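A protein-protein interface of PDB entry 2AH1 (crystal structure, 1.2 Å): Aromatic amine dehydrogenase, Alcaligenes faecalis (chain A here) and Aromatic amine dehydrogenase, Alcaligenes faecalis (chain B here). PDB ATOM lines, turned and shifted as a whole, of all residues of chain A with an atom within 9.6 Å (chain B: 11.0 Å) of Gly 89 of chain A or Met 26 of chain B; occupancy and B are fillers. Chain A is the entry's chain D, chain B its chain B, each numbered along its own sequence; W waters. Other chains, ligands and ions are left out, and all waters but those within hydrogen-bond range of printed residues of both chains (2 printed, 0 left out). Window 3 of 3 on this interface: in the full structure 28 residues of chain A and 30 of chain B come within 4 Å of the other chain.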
ATOM      1  N   GLY A  38      -9.553 -11.067   8.191  1.00  0.00           N
ATOM      2  CA  GLY A  38      -8.521 -10.313   7.467  1.00  0.00           C
ATOM      3  C   GLY A  38      -7.204 -11.029   7.491  1.00  0.00           C
ATOM      4  O   GLY A  38      -7.148 -12.208   7.772  1.00  0.00           O
ATOM      5  N   PHE A  39      -6.135 -10.319   7.195  1.00  0.00           N
ATOM      6  CA  PHE A  39      -4.787 -10.853   7.200  1.00  0.00           C
ATOM      7  C   PHE A  39      -4.090 -10.375   8.465  1.00  0.00           C
ATOM      8  O   PHE A  39      -4.132  -9.208   8.783  1.00  0.00           O
ATOM      9  CB  PHE A  39      -3.983 -10.331   5.983  1.00  0.00           C
ATOM     10  CG  PHE A  39      -4.668 -10.574   4.665  1.00  0.00           C
ATOM     11  CD1 PHE A  39      -5.187  -9.506   3.948  1.00  0.00           C
ATOM     12  CD2 PHE A  39      -4.820 -11.855   4.148  1.00  0.00           C
ATOM     13  CE1 PHE A  39      -5.822  -9.716   2.744  1.00  0.00           C
ATOM     14  CE2 PHE A  39      -5.456 -12.052   2.952  1.00  0.00           C
ATOM     15  CZ  PHE A  39      -5.958 -10.986   2.254  1.00  0.00           C
ATOM     16  N   LEU A  40      -3.419 -11.272   9.167  1.00  0.00           N
ATOM     17  CA  LEU A  40      -2.753 -10.842  10.398  1.00  0.00           C
ATOM     18  C   LEU A  40      -1.573  -9.934  10.103  1.00  0.00           C
ATOM     19  O   LEU A  40      -0.634 -10.325   9.415  1.00  0.00           O
ATOM     20  CB  LEU A  40      -2.265 -12.037  11.243  1.00  0.00           C
ATOM     21  CG  LEU A  40      -3.300 -13.068  11.624  1.00  0.00           C
ATOM     22  CD1 LEU A  40      -2.651 -14.206  12.370  1.00  0.00           C
ATOM     23  CD2 LEU A  40      -4.408 -12.448  12.436  1.00  0.00           C
ATOM     24  N   CYS A  41      -1.587  -8.707  10.649  1.00  0.00           N
ATOM     25  CA  CYS A  41      -0.483  -7.802  10.371  1.00  0.00           C
ATOM     26  C   CYS A  41       0.879  -8.304  10.794  1.00  0.00           C
ATOM     27  O   CYS A  41       1.884  -7.940  10.197  1.00  0.00           O
ATOM     28  CB  CYS A  41      -0.707  -6.416  10.954  1.00  0.00           C
ATOM     29  SG  CYS A  41      -2.007  -5.427  10.156  1.00  0.00           S
ATOM     30  N   CYS A  43       2.090 -11.085  10.223  1.00  0.00           N
ATOM     31  CA  CYS A  43       2.642 -11.842   9.087  1.00  0.00           C
ATOM     32  C   CYS A  43       2.997 -10.974   7.894  1.00  0.00           C
ATOM     33  O   CYS A  43       3.443 -11.480   6.865  1.00  0.00           O
ATOM     34  CB  CYS A  43       1.623 -12.846   8.606  1.00  0.00           C
ATOM     35  SG  CYS A  43       1.166 -14.065   9.856  1.00  0.00           S
ATOM     36  N   CYS A  44       2.789  -9.675   8.030  1.00  0.00           N
ATOM     37  CA  CYS A  44       2.809  -8.733   6.921  1.00  0.00           C
ATOM     38  C   CYS A  44       3.897  -7.686   7.102  1.00  0.00           C
ATOM     39  O   CYS A  44       3.900  -6.660   6.440  1.00  0.00           O
ATOM     40  CB  CYS A  44       1.434  -8.083   6.797  1.00  0.00           C
ATOM     41  SG  CYS A  44       0.124  -9.287   6.435  1.00  0.00           S
ATOM     42  N   PRO A  52       2.500  -2.571   9.299  1.00  0.00           N
ATOM     43  CA  PRO A  52       3.645  -2.728   8.382  1.00  0.00           C
ATOM     44  C   PRO A  52       4.072  -1.375   7.834  1.00  0.00           C
ATOM     45  O   PRO A  52       3.248  -0.481   7.680  1.00  0.00           O
ATOM     46  CB  PRO A  52       3.103  -3.632   7.294  1.00  0.00           C
ATOM     47  CG  PRO A  52       2.007  -4.427   7.978  1.00  0.00           C
ATOM     48  CD  PRO A  52       1.375  -3.451   8.919  1.00  0.00           C
ATOM     49  N   LYS A  85      -2.421   0.285   1.520  1.00  0.00           N
ATOM     50  CA  LYS A  85      -1.628  -0.627   0.683  1.00  0.00           C
ATOM     51  C   LYS A  85      -2.544  -1.771   0.344  1.00  0.00           C
ATOM     52  O   LYS A  85      -3.490  -2.079   1.029  1.00  0.00           O
ATOM     53  CB  LYS A  85      -0.362  -1.152   1.401  1.00  0.00           C
ATOM     54  CG  LYS A  85       0.770  -0.189   1.382  1.00  0.00           C
ATOM     55  CD  LYS A  85       2.092  -0.760   1.890  1.00  0.00           C
ATOM     56  CE  LYS A  85       3.154   0.235   1.579  1.00  0.00           C
ATOM     57  NZ  LYS A  85       4.461  -0.097   2.133  1.00  0.00           N
ATOM     58  N   THR A  86      -2.258  -2.412  -0.788  1.00  0.00           N
ATOM     59  CA  THR A  86      -3.080  -3.539  -1.288  1.00  0.00           C
ATOM     60  C   THR A  86      -2.884  -4.764  -0.369  1.00  0.00           C
ATOM     61  O   THR A  86      -1.994  -4.834   0.485  1.00  0.00           O
ATOM     62  CB  THR A  86      -2.765  -3.790  -2.734  1.00  0.00           C
ATOM     63  OG1 THR A  86      -1.340  -3.753  -2.881  1.00  0.00           O
ATOM     64  CG2 THR A  86      -3.401  -2.702  -3.627  1.00  0.00           C
ATOM     65  N   ALA A  87      -3.755  -5.736  -0.566  1.00  0.00           N
ATOM     66  CA  ALA A  87      -3.920  -6.823   0.360  1.00  0.00           C
ATOM     67  C   ALA A  87      -2.622  -7.526   0.652  1.00  0.00           C
ATOM     68  O   ALA A  87      -1.916  -7.967  -0.262  1.00  0.00           O
ATOM     69  CB  ALA A  87      -4.888  -7.824  -0.263  1.00  0.00           C
ATOM     70  N   CYS A  88      -2.317  -7.668   1.945  1.00  0.00           N
ATOM     71  CA  CYS A  88      -1.127  -8.380   2.296  1.00  0.00           C
ATOM     72  C   CYS A  88      -1.095  -9.825   1.828  1.00  0.00           C
ATOM     73  O   CYS A  88      -0.042 -10.293   1.402  1.00  0.00           O
ATOM     74  CB  CYS A  88      -0.982  -8.360   3.813  1.00  0.00           C
ATOM     75  SG  CYS A  88       0.306  -9.489   4.401  1.00  0.00           S
ATOM     76  N   GLY A  89      -2.216 -10.529   1.951  1.00  0.00           N
ATOM     77  CA  GLY A  89      -2.331 -11.883   1.440  1.00  0.00           C
ATOM     78  C   GLY A  89      -1.785 -12.996   2.283  1.00  0.00           C
ATOM     79  O   GLY A  89      -1.871 -14.152   1.878  1.00  0.00           O
ATOM     80  N   ARG A  90      -1.230 -12.687   3.448  1.00  0.00           N
ATOM     81  CA  ARG A  90      -0.650 -13.692   4.310  1.00  0.00           C
ATOM     82  C   ARG A  90      -1.465 -13.808   5.585  1.00  0.00           C
ATOM     83  O   ARG A  90      -2.004 -12.832   6.065  1.00  0.00           O
ATOM     84  CB  ARG A  90       0.801 -13.314   4.624  1.00  0.00           C
ATOM     85  CG  ARG A  90       1.681 -13.447   3.399  1.00  0.00           C
ATOM     86  CD  ARG A  90       2.620 -12.349   3.142  1.00  0.00           C
ATOM     87  NE  ARG A  90       3.457 -12.732   2.001  1.00  0.00           N
ATOM     88  CZ  ARG A  90       3.134 -12.648   0.716  1.00  0.00           C
ATOM     89  NH1 ARG A  90       1.957 -12.176   0.323  1.00  0.00           N
ATOM     90  NH2 ARG A  90       4.011 -13.054  -0.192  1.00  0.00           N
ATOM     91  N   CYS A  91      -1.544 -15.027   6.095  1.00  0.00           N
ATOM     92  CA  CYS A  91      -2.234 -15.306   7.365  1.00  0.00           C
ATOM     93  C   CYS A  91      -3.658 -14.799   7.350  1.00  0.00           C
ATOM     94  O   CYS A  91      -4.067 -14.033   8.229  1.00  0.00           O
ATOM     95  CB  CYS A  91      -1.472 -14.732   8.572  1.00  0.00           C
ATOM     96  SG  CYS A  91       0.186 -15.441   8.709  1.00  0.00           S
ATOM     97  N   GLN A  92      -4.429 -15.222   6.357  1.00  0.00           N
ATOM     98  CA  GLN A  92      -5.838 -14.882   6.320  1.00  0.00           C
ATOM     99  C   GLN A  92      -6.552 -15.667   7.406  1.00  0.00           C
ATOM    100  O   GLN A  92      -6.383 -16.876   7.527  1.00  0.00           O
ATOM    101  CB  GLN A  92      -6.501 -15.158   4.959  1.00  0.00           C
ATOM    102  CG  GLN A  92      -7.872 -14.480   4.872  1.00  0.00           C
ATOM    103  CD  GLN A  92      -8.600 -14.628   3.542  1.00  0.00           C
ATOM    104  OE1 GLN A  92      -9.825 -14.387   3.456  1.00  0.00           O
ATOM    105  NE2 GLN A  92      -7.876 -15.017   2.520  1.00  0.00           N
ATOM    106  N   CYS A  93      -7.348 -14.964   8.191  1.00  0.00           N
ATOM    107  CA  CYS A  93      -8.136 -15.582   9.269  1.00  0.00           C
ATOM    108  C   CYS A  93      -9.576 -15.138   9.129  1.00  0.00           C
ATOM    109  O   CYS A  93      -9.855 -14.072   8.593  1.00  0.00           O
ATOM    110  CB  CYS A  93      -7.584 -15.143  10.634  1.00  0.00           C
ATOM    111  SG  CYS A  93      -5.875 -15.657  10.911  1.00  0.00           S
ATOM    112  N   THR A 121      -7.970   1.335   1.005  1.00  0.00           N
ATOM    113  CA  THR A 121      -7.533   0.010   0.586  1.00  0.00           C
ATOM    114  C   THR A 121      -7.068  -0.766   1.810  1.00  0.00           C
ATOM    115  O   THR A 121      -6.284  -0.274   2.624  1.00  0.00           O
ATOM    116  CB  THR A 121      -6.394   0.100  -0.433  1.00  0.00           C
ATOM    117  OG1 THR A 121      -6.737   1.000  -1.503  1.00  0.00           O
ATOM    118  CG2 THR A 121      -6.107  -1.247  -1.046  1.00  0.00           C
ATOM    119  N   PHE A 122      -7.580  -1.977   1.933  1.00  0.00           N
ATOM    120  CA  PHE A 122      -7.330  -2.802   3.101  1.00  0.00           C
ATOM    121  C   PHE A 122      -6.045  -3.595   2.947  1.00  0.00           C
ATOM    122  O   PHE A 122      -5.870  -4.322   1.974  1.00  0.00           O
ATOM    123  CB  PHE A 122      -8.493  -3.765   3.330  1.00  0.00           C
ATOM    124  CG  PHE A 122      -8.198  -4.795   4.374  1.00  0.00           C
ATOM    125  CD1 PHE A 122      -8.189  -4.470   5.719  1.00  0.00           C
ATOM    126  CD2 PHE A 122      -7.922  -6.100   4.019  1.00  0.00           C
ATOM    127  CE1 PHE A 122      -7.910  -5.437   6.669  1.00  0.00           C
ATOM    128  CE2 PHE A 122      -7.638  -7.053   4.982  1.00  0.00           C
ATOM    129  CZ  PHE A 122      -7.636  -6.723   6.295  1.00  0.00           C
ATOM    130  N   HIS A 123      -5.157  -3.456   3.923  1.00  0.00           N
ATOM    131  CA  HIS A 123      -3.887  -4.136   3.928  1.00  0.00           C
ATOM    132  C   HIS A 123      -3.839  -5.341   4.859  1.00  0.00           C
ATOM    133  O   HIS A 123      -3.529  -6.456   4.441  1.00  0.00           O
ATOM    134  CB  HIS A 123      -2.751  -3.151   4.210  1.00  0.00           C
ATOM    135  CG  HIS A 123      -1.401  -3.750   4.125  1.00  0.00           C
ATOM    136  ND1 HIS A 123      -0.948  -4.404   3.011  1.00  0.00           N
ATOM    137  CD2 HIS A 123      -0.395  -3.813   5.023  1.00  0.00           C
ATOM    138  CE1 HIS A 123       0.285  -4.832   3.233  1.00  0.00           C
ATOM    139  NE2 HIS A 123       0.646  -4.496   4.449  1.00  0.00           N
ATOM    140  N   CYS A 124      -4.104  -5.113   6.140  1.00  0.00           N
ATOM    141  CA  CYS A 124      -4.074  -6.152   7.181  1.00  0.00           C
ATOM    142  C   CYS A 124      -4.805  -5.708   8.423  1.00  0.00           C
ATOM    143  O   CYS A 124      -5.111  -4.530   8.569  1.00  0.00           O
ATOM    144  CB  CYS A 124      -2.649  -6.622   7.478  1.00  0.00           C
ATOM    145  SG  CYS A 124      -1.558  -5.391   8.164  1.00  0.00           S
ATOM    146  N   THR A 125      -5.089  -6.689   9.253  1.00  0.00           N
ATOM    147  CA  THR A 125      -5.770  -6.471  10.543  1.00  0.00           C
ATOM    148  C   THR A 125      -4.828  -6.631  11.742  1.00  0.00           C
ATOM    149  O   THR A 125      -4.058  -7.586  11.805  1.00  0.00           O
ATOM    150  CB  THR A 125      -6.857  -7.532  10.691  1.00  0.00           C
ATOM    151  OG1 THR A 125      -7.697  -7.538   9.528  1.00  0.00           O
ATOM    152  CG2 THR A 125      -7.768  -7.233  11.890  1.00  0.00           C
ATOM    153  N   ASP B  22     -17.323 -11.830  -7.740  1.00  0.00           N
ATOM    154  CA  ASP B  22     -16.045 -12.317  -7.237  1.00  0.00           C
ATOM    155  C   ASP B  22     -15.333 -11.172  -6.548  1.00  0.00           C
ATOM    156  O   ASP B  22     -14.835 -10.258  -7.202  1.00  0.00           O
ATOM    157  CB  ASP B  22     -15.189 -12.915  -8.351  1.00  0.00           C
ATOM    158  CG  ASP B  22     -14.065 -13.749  -7.813  1.00  0.00           C
ATOM    159  OD1 ASP B  22     -13.844 -13.744  -6.553  1.00  0.00           O
ATOM    160  OD2 ASP B  22     -13.380 -14.424  -8.610  1.00  0.00           O
ATOM    161  N   SER B  23     -15.270 -11.222  -5.224  1.00  0.00           N
ATOM    162  CA  SER B  23     -14.556 -10.186  -4.488  1.00  0.00           C
ATOM    163  C   SER B  23     -13.064 -10.224  -4.741  1.00  0.00           C
ATOM    164  O   SER B  23     -12.404  -9.204  -4.612  1.00  0.00           O
ATOM    165  CB  SER B  23     -14.802 -10.293  -2.969  1.00  0.00           C
ATOM    166  OG  SER B  23     -14.096 -11.391  -2.392  1.00  0.00           O
ATOM    167  N   VAL B  24     -12.523 -11.395  -5.065  1.00  0.00           N
ATOM    168  CA  VAL B  24     -11.078 -11.543  -5.227  1.00  0.00           C
ATOM    169  C   VAL B  24     -10.379 -10.919  -4.019  1.00  0.00           C
ATOM    170  O   VAL B  24      -9.507 -10.081  -4.150  1.00  0.00           O
ATOM    171  CB  VAL B  24     -10.517 -10.961  -6.567  1.00  0.00           C
ATOM    172  CG1 VAL B  24      -9.112 -11.469  -6.839  1.00  0.00           C
ATOM    173  CG2 VAL B  24     -11.402 -11.338  -7.717  1.00  0.00           C
ATOM    174  N   PHE B  25     -10.748 -11.369  -2.830  1.00  0.00           N
ATOM    175  CA  PHE B  25     -10.256 -10.754  -1.609  1.00  0.00           C
ATOM    176  C   PHE B  25      -8.731 -10.711  -1.559  1.00  0.00           C
ATOM    177  O   PHE B  25      -8.178  -9.756  -1.021  1.00  0.00           O
ATOM    178  CB  PHE B  25     -10.855 -11.467  -0.394  1.00  0.00           C
ATOM    179  CG  PHE B  25     -10.667 -10.731   0.903  1.00  0.00           C
ATOM    180  CD1 PHE B  25     -11.460  -9.642   1.250  1.00  0.00           C
ATOM    181  CD2 PHE B  25      -9.679 -11.129   1.781  1.00  0.00           C
ATOM    182  CE1 PHE B  25     -11.267  -8.975   2.466  1.00  0.00           C
ATOM    183  CE2 PHE B  25      -9.494 -10.476   2.969  1.00  0.00           C
ATOM    184  CZ  PHE B  25     -10.285  -9.400   3.304  1.00  0.00           C
ATOM    185  N   MET B  26      -8.039 -11.708  -2.110  1.00  0.00           N
ATOM    186  CA  MET B  26      -6.582 -11.676  -2.080  1.00  0.00           C
ATOM    187  C   MET B  26      -6.000 -10.522  -2.903  1.00  0.00           C
ATOM    188  O   MET B  26      -4.851 -10.111  -2.706  1.00  0.00           O
ATOM    189  CB  MET B  26      -6.011 -12.977  -2.633  1.00  0.00           C
ATOM    190  CG  MET B  26      -6.132 -14.161  -1.694  1.00  0.00           C
ATOM    191  SD  MET B  26      -5.054 -14.066  -0.260  1.00  0.00           S
ATOM    192  CE  MET B  26      -3.491 -14.309  -1.108  1.00  0.00           C
ATOM    193  N   HIS B  27      -6.813 -10.015  -3.832  1.00  0.00           N
ATOM    194  CA  HIS B  27      -6.468  -8.872  -4.692  1.00  0.00           C
ATOM    195  C   HIS B  27      -7.709  -8.019  -4.887  1.00  0.00           C
ATOM    196  O   HIS B  27      -8.187  -7.862  -6.024  1.00  0.00           O
ATOM    197  CB  HIS B  27      -5.844  -9.330  -6.022  1.00  0.00           C
ATOM    198  CG  HIS B  27      -4.617 -10.121  -5.779  1.00  0.00           C
ATOM    199  ND1 HIS B  27      -3.462  -9.543  -5.302  1.00  0.00           N
ATOM    200  CD2 HIS B  27      -4.364 -11.448  -5.882  1.00  0.00           C
ATOM    201  CE1 HIS B  27      -2.549 -10.476  -5.133  1.00  0.00           C
ATOM    202  NE2 HIS B  27      -3.072 -11.647  -5.464  1.00  0.00           N
ATOM    203  N   LEU B  28      -8.200  -7.460  -3.772  1.00  0.00           N
ATOM    204  CA  LEU B  28      -9.531  -6.918  -3.701  1.00  0.00           C
ATOM    205  C   LEU B  28      -9.726  -5.675  -4.572  1.00  0.00           C
ATOM    206  O   LEU B  28     -10.853  -5.283  -4.809  1.00  0.00           O
ATOM    207  CB  LEU B  28      -9.841  -6.617  -2.239  1.00  0.00           C
ATOM    208  CG  LEU B  28     -11.218  -6.109  -1.808  1.00  0.00           C
ATOM    209  CD1 LEU B  28     -12.303  -7.076  -2.267  1.00  0.00           C
ATOM    210  CD2 LEU B  28     -11.277  -5.929  -0.298  1.00  0.00           C
ATOM    211  N   THR B  29      -8.642  -5.055  -5.032  1.00  0.00           N
ATOM    212  CA  THR B  29      -8.737  -3.963  -5.987  1.00  0.00           C
ATOM    213  C   THR B  29      -9.114  -4.423  -7.396  1.00  0.00           C
ATOM    214  O   THR B  29      -9.332  -3.577  -8.261  1.00  0.00           O
ATOM    215  CB  THR B  29      -7.479  -3.095  -6.083  1.00  0.00           C
ATOM    216  OG1 THR B  29      -6.386  -3.846  -6.633  1.00  0.00           O
ATOM    217  CG2 THR B  29      -7.076  -2.481  -4.719  1.00  0.00           C
ATOM    218  N   GLU B  30      -9.174  -5.740  -7.631  1.00  0.00           N
ATOM    219  CA  GLU B  30      -9.533  -6.273  -8.946  1.00  0.00           C
ATOM    220  C   GLU B  30     -10.718  -7.229  -8.856  1.00  0.00           C
ATOM    221  O   GLU B  30     -10.768  -8.246  -9.553  1.00  0.00           O
ATOM    222  CB  GLU B  30      -8.336  -6.926  -9.680  1.00  0.00           C
ATOM    223  CG  GLU B  30      -8.471  -6.872 -11.177  1.00  0.00           C
ATOM    224  CD  GLU B  30      -7.468  -7.702 -11.910  1.00  0.00           C
ATOM    225  OE1 GLU B  30      -6.390  -7.188 -12.242  1.00  0.00           O
ATOM    226  OE2 GLU B  30      -7.785  -8.880 -12.188  1.00  0.00           O
ATOM    227  N   SER B  31     -11.675  -6.884  -8.020  1.00  0.00           N
ATOM    228  CA  SER B  31     -12.933  -7.580  -7.945  1.00  0.00           C
ATOM    229  C   SER B  31     -13.631  -7.497  -9.308  1.00  0.00           C
ATOM    230  O   SER B  31     -13.373  -6.595 -10.087  1.00  0.00           O
ATOM    231  CB  SER B  31     -13.813  -7.008  -6.837  1.00  0.00           C
ATOM    232  OG  SER B  31     -14.313  -5.713  -7.147  1.00  0.00           O
ATOM    233  N   ARG B  32     -14.525  -8.430  -9.562  1.00  0.00           N
ATOM    234  CA  ARG B  32     -15.248  -8.458 -10.842  1.00  0.00           C
ATOM    235  C   ARG B  32     -16.460  -9.326 -10.730  1.00  0.00           C
ATOM    236  O   ARG B  32     -16.568 -10.184  -9.838  1.00  0.00           O
ATOM    237  CB  ARG B  32     -14.364  -8.954 -12.014  1.00  0.00           C
ATOM    238  CG  ARG B  32     -14.042 -10.434 -11.959  1.00  0.00           C
ATOM    239  CD  ARG B  32     -12.836 -10.851 -11.119  1.00  0.00           C
ATOM    240  NE  ARG B  32     -11.603 -10.341 -11.671  1.00  0.00           N
ATOM    241  CZ  ARG B  32     -11.024 -10.822 -12.767  1.00  0.00           C
ATOM    242  NH1 ARG B  32     -11.534 -11.850 -13.415  1.00  0.00           N
ATOM    243  NH2 ARG B  32      -9.913 -10.297 -13.231  1.00  0.00           N
ATOM    244  N   ALA B  50     -13.262  -3.029  -9.797  1.00  0.00           N
ATOM    245  CA  ALA B  50     -12.300  -2.284  -8.980  1.00  0.00           C
ATOM    246  C   ALA B  50     -12.290  -2.782  -7.537  1.00  0.00           C
ATOM    247  O   ALA B  50     -12.278  -4.008  -7.327  1.00  0.00           O
ATOM    248  CB  ALA B  50     -12.528  -0.785  -9.108  1.00  0.00           C
ATOM    249  N   PHE B  51     -12.246  -1.887  -6.552  1.00  0.00           N
ATOM    250  CA  PHE B  51     -12.105  -2.311  -5.166  1.00  0.00           C
ATOM    251  C   PHE B  51     -13.435  -2.736  -4.567  1.00  0.00           C
ATOM    252  O   PHE B  51     -14.342  -1.926  -4.449  1.00  0.00           O
ATOM    253  CB  PHE B  51     -11.510  -1.191  -4.292  1.00  0.00           C
ATOM    254  CG  PHE B  51     -11.351  -1.560  -2.856  1.00  0.00           C
ATOM    255  CD1 PHE B  51     -10.303  -2.363  -2.469  1.00  0.00           C
ATOM    256  CD2 PHE B  51     -12.240  -1.109  -1.891  1.00  0.00           C
ATOM    257  CE1 PHE B  51     -10.158  -2.699  -1.164  1.00  0.00           C
ATOM    258  CE2 PHE B  51     -12.072  -1.461  -0.576  1.00  0.00           C
ATOM    259  CZ  PHE B  51     -11.035  -2.255  -0.215  1.00  0.00           C
ATOM    260  N   ASN B  52     -13.551  -4.009  -4.202  1.00  0.00           N
ATOM    261  CA  ASN B  52     -14.735  -4.493  -3.476  1.00  0.00           C
ATOM    262  C   ASN B  52     -16.040  -4.095  -4.112  1.00  0.00           C
ATOM    263  O   ASN B  52     -16.883  -3.457  -3.477  1.00  0.00           O
ATOM    264  CB  ASN B  52     -14.692  -3.999  -2.026  1.00  0.00           C
ATOM    265  CG  ASN B  52     -15.840  -4.495  -1.172  1.00  0.00           C
ATOM    266  OD1 ASN B  52     -16.270  -5.662  -1.232  1.00  0.00           O
ATOM    267  ND2 ASN B  52     -16.333  -3.617  -0.355  1.00  0.00           N
ATOM    268  N   LEU B 107     -18.450  -7.246   2.669  1.00  0.00           N
ATOM    269  CA  LEU B 107     -18.825  -8.448   1.952  1.00  0.00           C
ATOM    270  C   LEU B 107     -20.198  -8.317   1.313  1.00  0.00           C
ATOM    271  O   LEU B 107     -21.028  -7.511   1.724  1.00  0.00           O
ATOM    272  CB  LEU B 107     -18.797  -9.657   2.889  1.00  0.00           C
ATOM    273  CG  LEU B 107     -17.480  -9.897   3.620  1.00  0.00           C
ATOM    274  CD1 LEU B 107     -17.584 -11.155   4.442  1.00  0.00           C
ATOM    275  CD2 LEU B 107     -16.256  -9.936   2.729  1.00  0.00           C
ATOM    276  N   GLY B 324     -18.085 -20.290  -2.200  1.00  0.00           N
ATOM    277  CA  GLY B 324     -16.971 -19.348  -2.303  1.00  0.00           C
ATOM    278  C   GLY B 324     -16.312 -19.397  -3.671  1.00  0.00           C
ATOM    279  O   GLY B 324     -15.797 -18.388  -4.150  1.00  0.00           O
ATOM    280  N   ALA B 347     -15.516 -18.563  -9.302  1.00  0.00           N
ATOM    281  CA  ALA B 347     -14.931 -17.421  -8.642  1.00  0.00           C
ATOM    282  C   ALA B 347     -13.816 -17.895  -7.766  1.00  0.00           C
ATOM    283  O   ALA B 347     -13.747 -19.069  -7.419  1.00  0.00           O
ATOM    284  CB  ALA B 347     -15.975 -16.711  -7.783  1.00  0.00           C
ATOM    285  N   GLU B 348     -12.959 -16.962  -7.364  1.00  0.00           N
ATOM    286  CA  GLU B 348     -11.966 -17.209  -6.326  1.00  0.00           C
ATOM    287  C   GLU B 348     -12.492 -16.931  -4.924  1.00  0.00           C
ATOM    288  O   GLU B 348     -12.146 -17.641  -4.002  1.00  0.00           O
ATOM    289  CB  GLU B 348     -10.720 -16.378  -6.587  1.00  0.00           C
ATOM    290  CG  GLU B 348      -9.984 -16.842  -7.837  1.00  0.00           C
ATOM    291  CD  GLU B 348      -8.771 -16.001  -8.095  1.00  0.00           C
ATOM    292  OE1 GLU B 348      -7.711 -16.244  -7.479  1.00  0.00           O
ATOM    293  OE2 GLU B 348      -8.895 -15.079  -8.874  1.00  0.00           O
ATOM    294  N   ALA B 349     -13.320 -15.909  -4.767  1.00  0.00           N
ATOM    295  CA  ALA B 349     -13.805 -15.530  -3.433  1.00  0.00           C
ATOM    296  C   ALA B 349     -15.132 -14.814  -3.586  1.00  0.00           C
ATOM    297  O   ALA B 349     -15.217 -13.579  -3.486  1.00  0.00           O
ATOM    298  CB  ALA B 349     -12.779 -14.635  -2.704  1.00  0.00           C
ATOM    299  N   SER B 350     -16.186 -15.588  -3.824  1.00  0.00           N
ATOM    300  CA  SER B 350     -17.513 -15.018  -3.974  1.00  0.00           C
ATOM    301  C   SER B 350     -18.431 -15.472  -2.877  1.00  0.00           C
ATOM    302  O   SER B 350     -18.465 -16.656  -2.555  1.00  0.00           O
ATOM    303  CB  SER B 350     -18.134 -15.449  -5.291  1.00  0.00           C
ATOM    304  OG  SER B 350     -19.437 -14.916  -5.429  1.00  0.00           O
HETATM  305  O   HOH W   1      -2.419 -10.516  -1.519  1.00  0.00           O
HETATM  306  O   HOH W   2      -5.926 -16.900   2.024  1.00  0.00           O
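The backbone NH (N) of Thr 125 of chain A lies within hydrogen-bond range of the backbone carbonyl oxygen (O) of Phe 39 of chain A, at 2.7 Å. O of Thr 86 of chain A lies within hydrogen-bond range of ND1 of His 123 of chain A (2.8 Å). OG of Ser 23 of chain B sits close to N of Phe 25 of chain B, at 3.4 Å. SG of Cys 41 of chain A forms a disulfide with SG of Cys 124 of chain A (2.0 Å). SG of Cys 91 of chain A forms a disulfide with SG of Cys 43 of chain A, 2.0 Å away. SG of Cys 44 of chain A is disulfide-bonded to SG of Cys 88 of chain A (2.1 Å).
Of the 21 printed residues of chain A, 7 touch a printed residue of chain B. Along chain A the printed residues that touch a printed residue of chain B span positions 39 to 122. Among the printed residues, 9 pairs touch across the chains. Among the printed residues, no Asp or Glu carboxylate lies within 4 Å of a Lys or Arg side-chain nitrogen of the other chain.
CE2 of Phe 25 of chain B touches CZ of Phe 39 of chain A, at 3.6 Å. Met 26 of chain B touches Phe 39 of chain A. CG2 of Thr 86 of chain A touches CG2 of Thr 29 of chain B, 3.8 Å away. Ala 87 of chain A touches Phe 25 of chain B (CB to O, 3.9 Å). Ala 87 of chain A touches Met 26 of chain B. Gly 89 of chain A touches Met 26 of chain B (O to CE, 3.4 Å). Gln 92 of chain A touches Phe 25 of chain B (OE1 to CD2, 3.7 Å). Thr 121 of chain A touches Thr 29 of chain B (CG2 to CG2, 3.99 Å). Phe 122 of chain A touches Phe 25 of chain B (CE2 to CZ, 3.9 Å).
Water W1 lies within hydrogen-bond range of O of Met 26 of chain B (2.7 Å), O of Ala 87 of chain A (2.9 Å) and N of Gly 89 of chain A (3.5 Å). Water W2 bridges the side-chain amide nitrogen (NE2) of Gln 92 of chain A and the side-chain sulfur (SD) of Met 26 of chain B.
Of the printed residues of chain B, Gly 89 of chain A touches Met 26 (3.4 Å). Of chain A, only Phe 39 (3.8 Å), Ala 87 (3.3 Å) and Gly 89 (3.4 Å) come within 4 Å of Met 26 of chain B. Of chain B, only Phe 25 and Met 26 come within 4 Å of Ala 87 of chain A. No residue of chain B comes within 4 Å of Cys 88 of chain A. No residue of chain B comes within 4 Å of Arg 90 of chain A. No residue of chain A comes within 4 Å of His 27 of chain B. Printed residues of chain B within 4 Å of Gln 92 of chain A: Phe 25 (3.7 Å). Printed residues of chain B within 4 Å of Phe 122 of chain A: Phe 25 (3.9 Å). Printed residues of chain A within 4 Å of Thr 29 of chain B: Thr 86 and Thr 121. Of the printed residues of chain B, Thr 121 of chain A touches Thr 29. Gly 324 of chain B touches none of the printed residues of chain A. Cys 91 of chain A touches none of the printed residues of chain B. The nearest residue of chain B that does not touch Gly 89 of chain A is Phe 25 of chain B (6.7 Å). The nearest residue of chain A that does not touch Met 26 of chain B is Gln 92 of chain A (4.1 Å). The nearest printed residue of chain B that does not touch Phe 39 of chain A is His 27 of chain B (6.2 Å).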
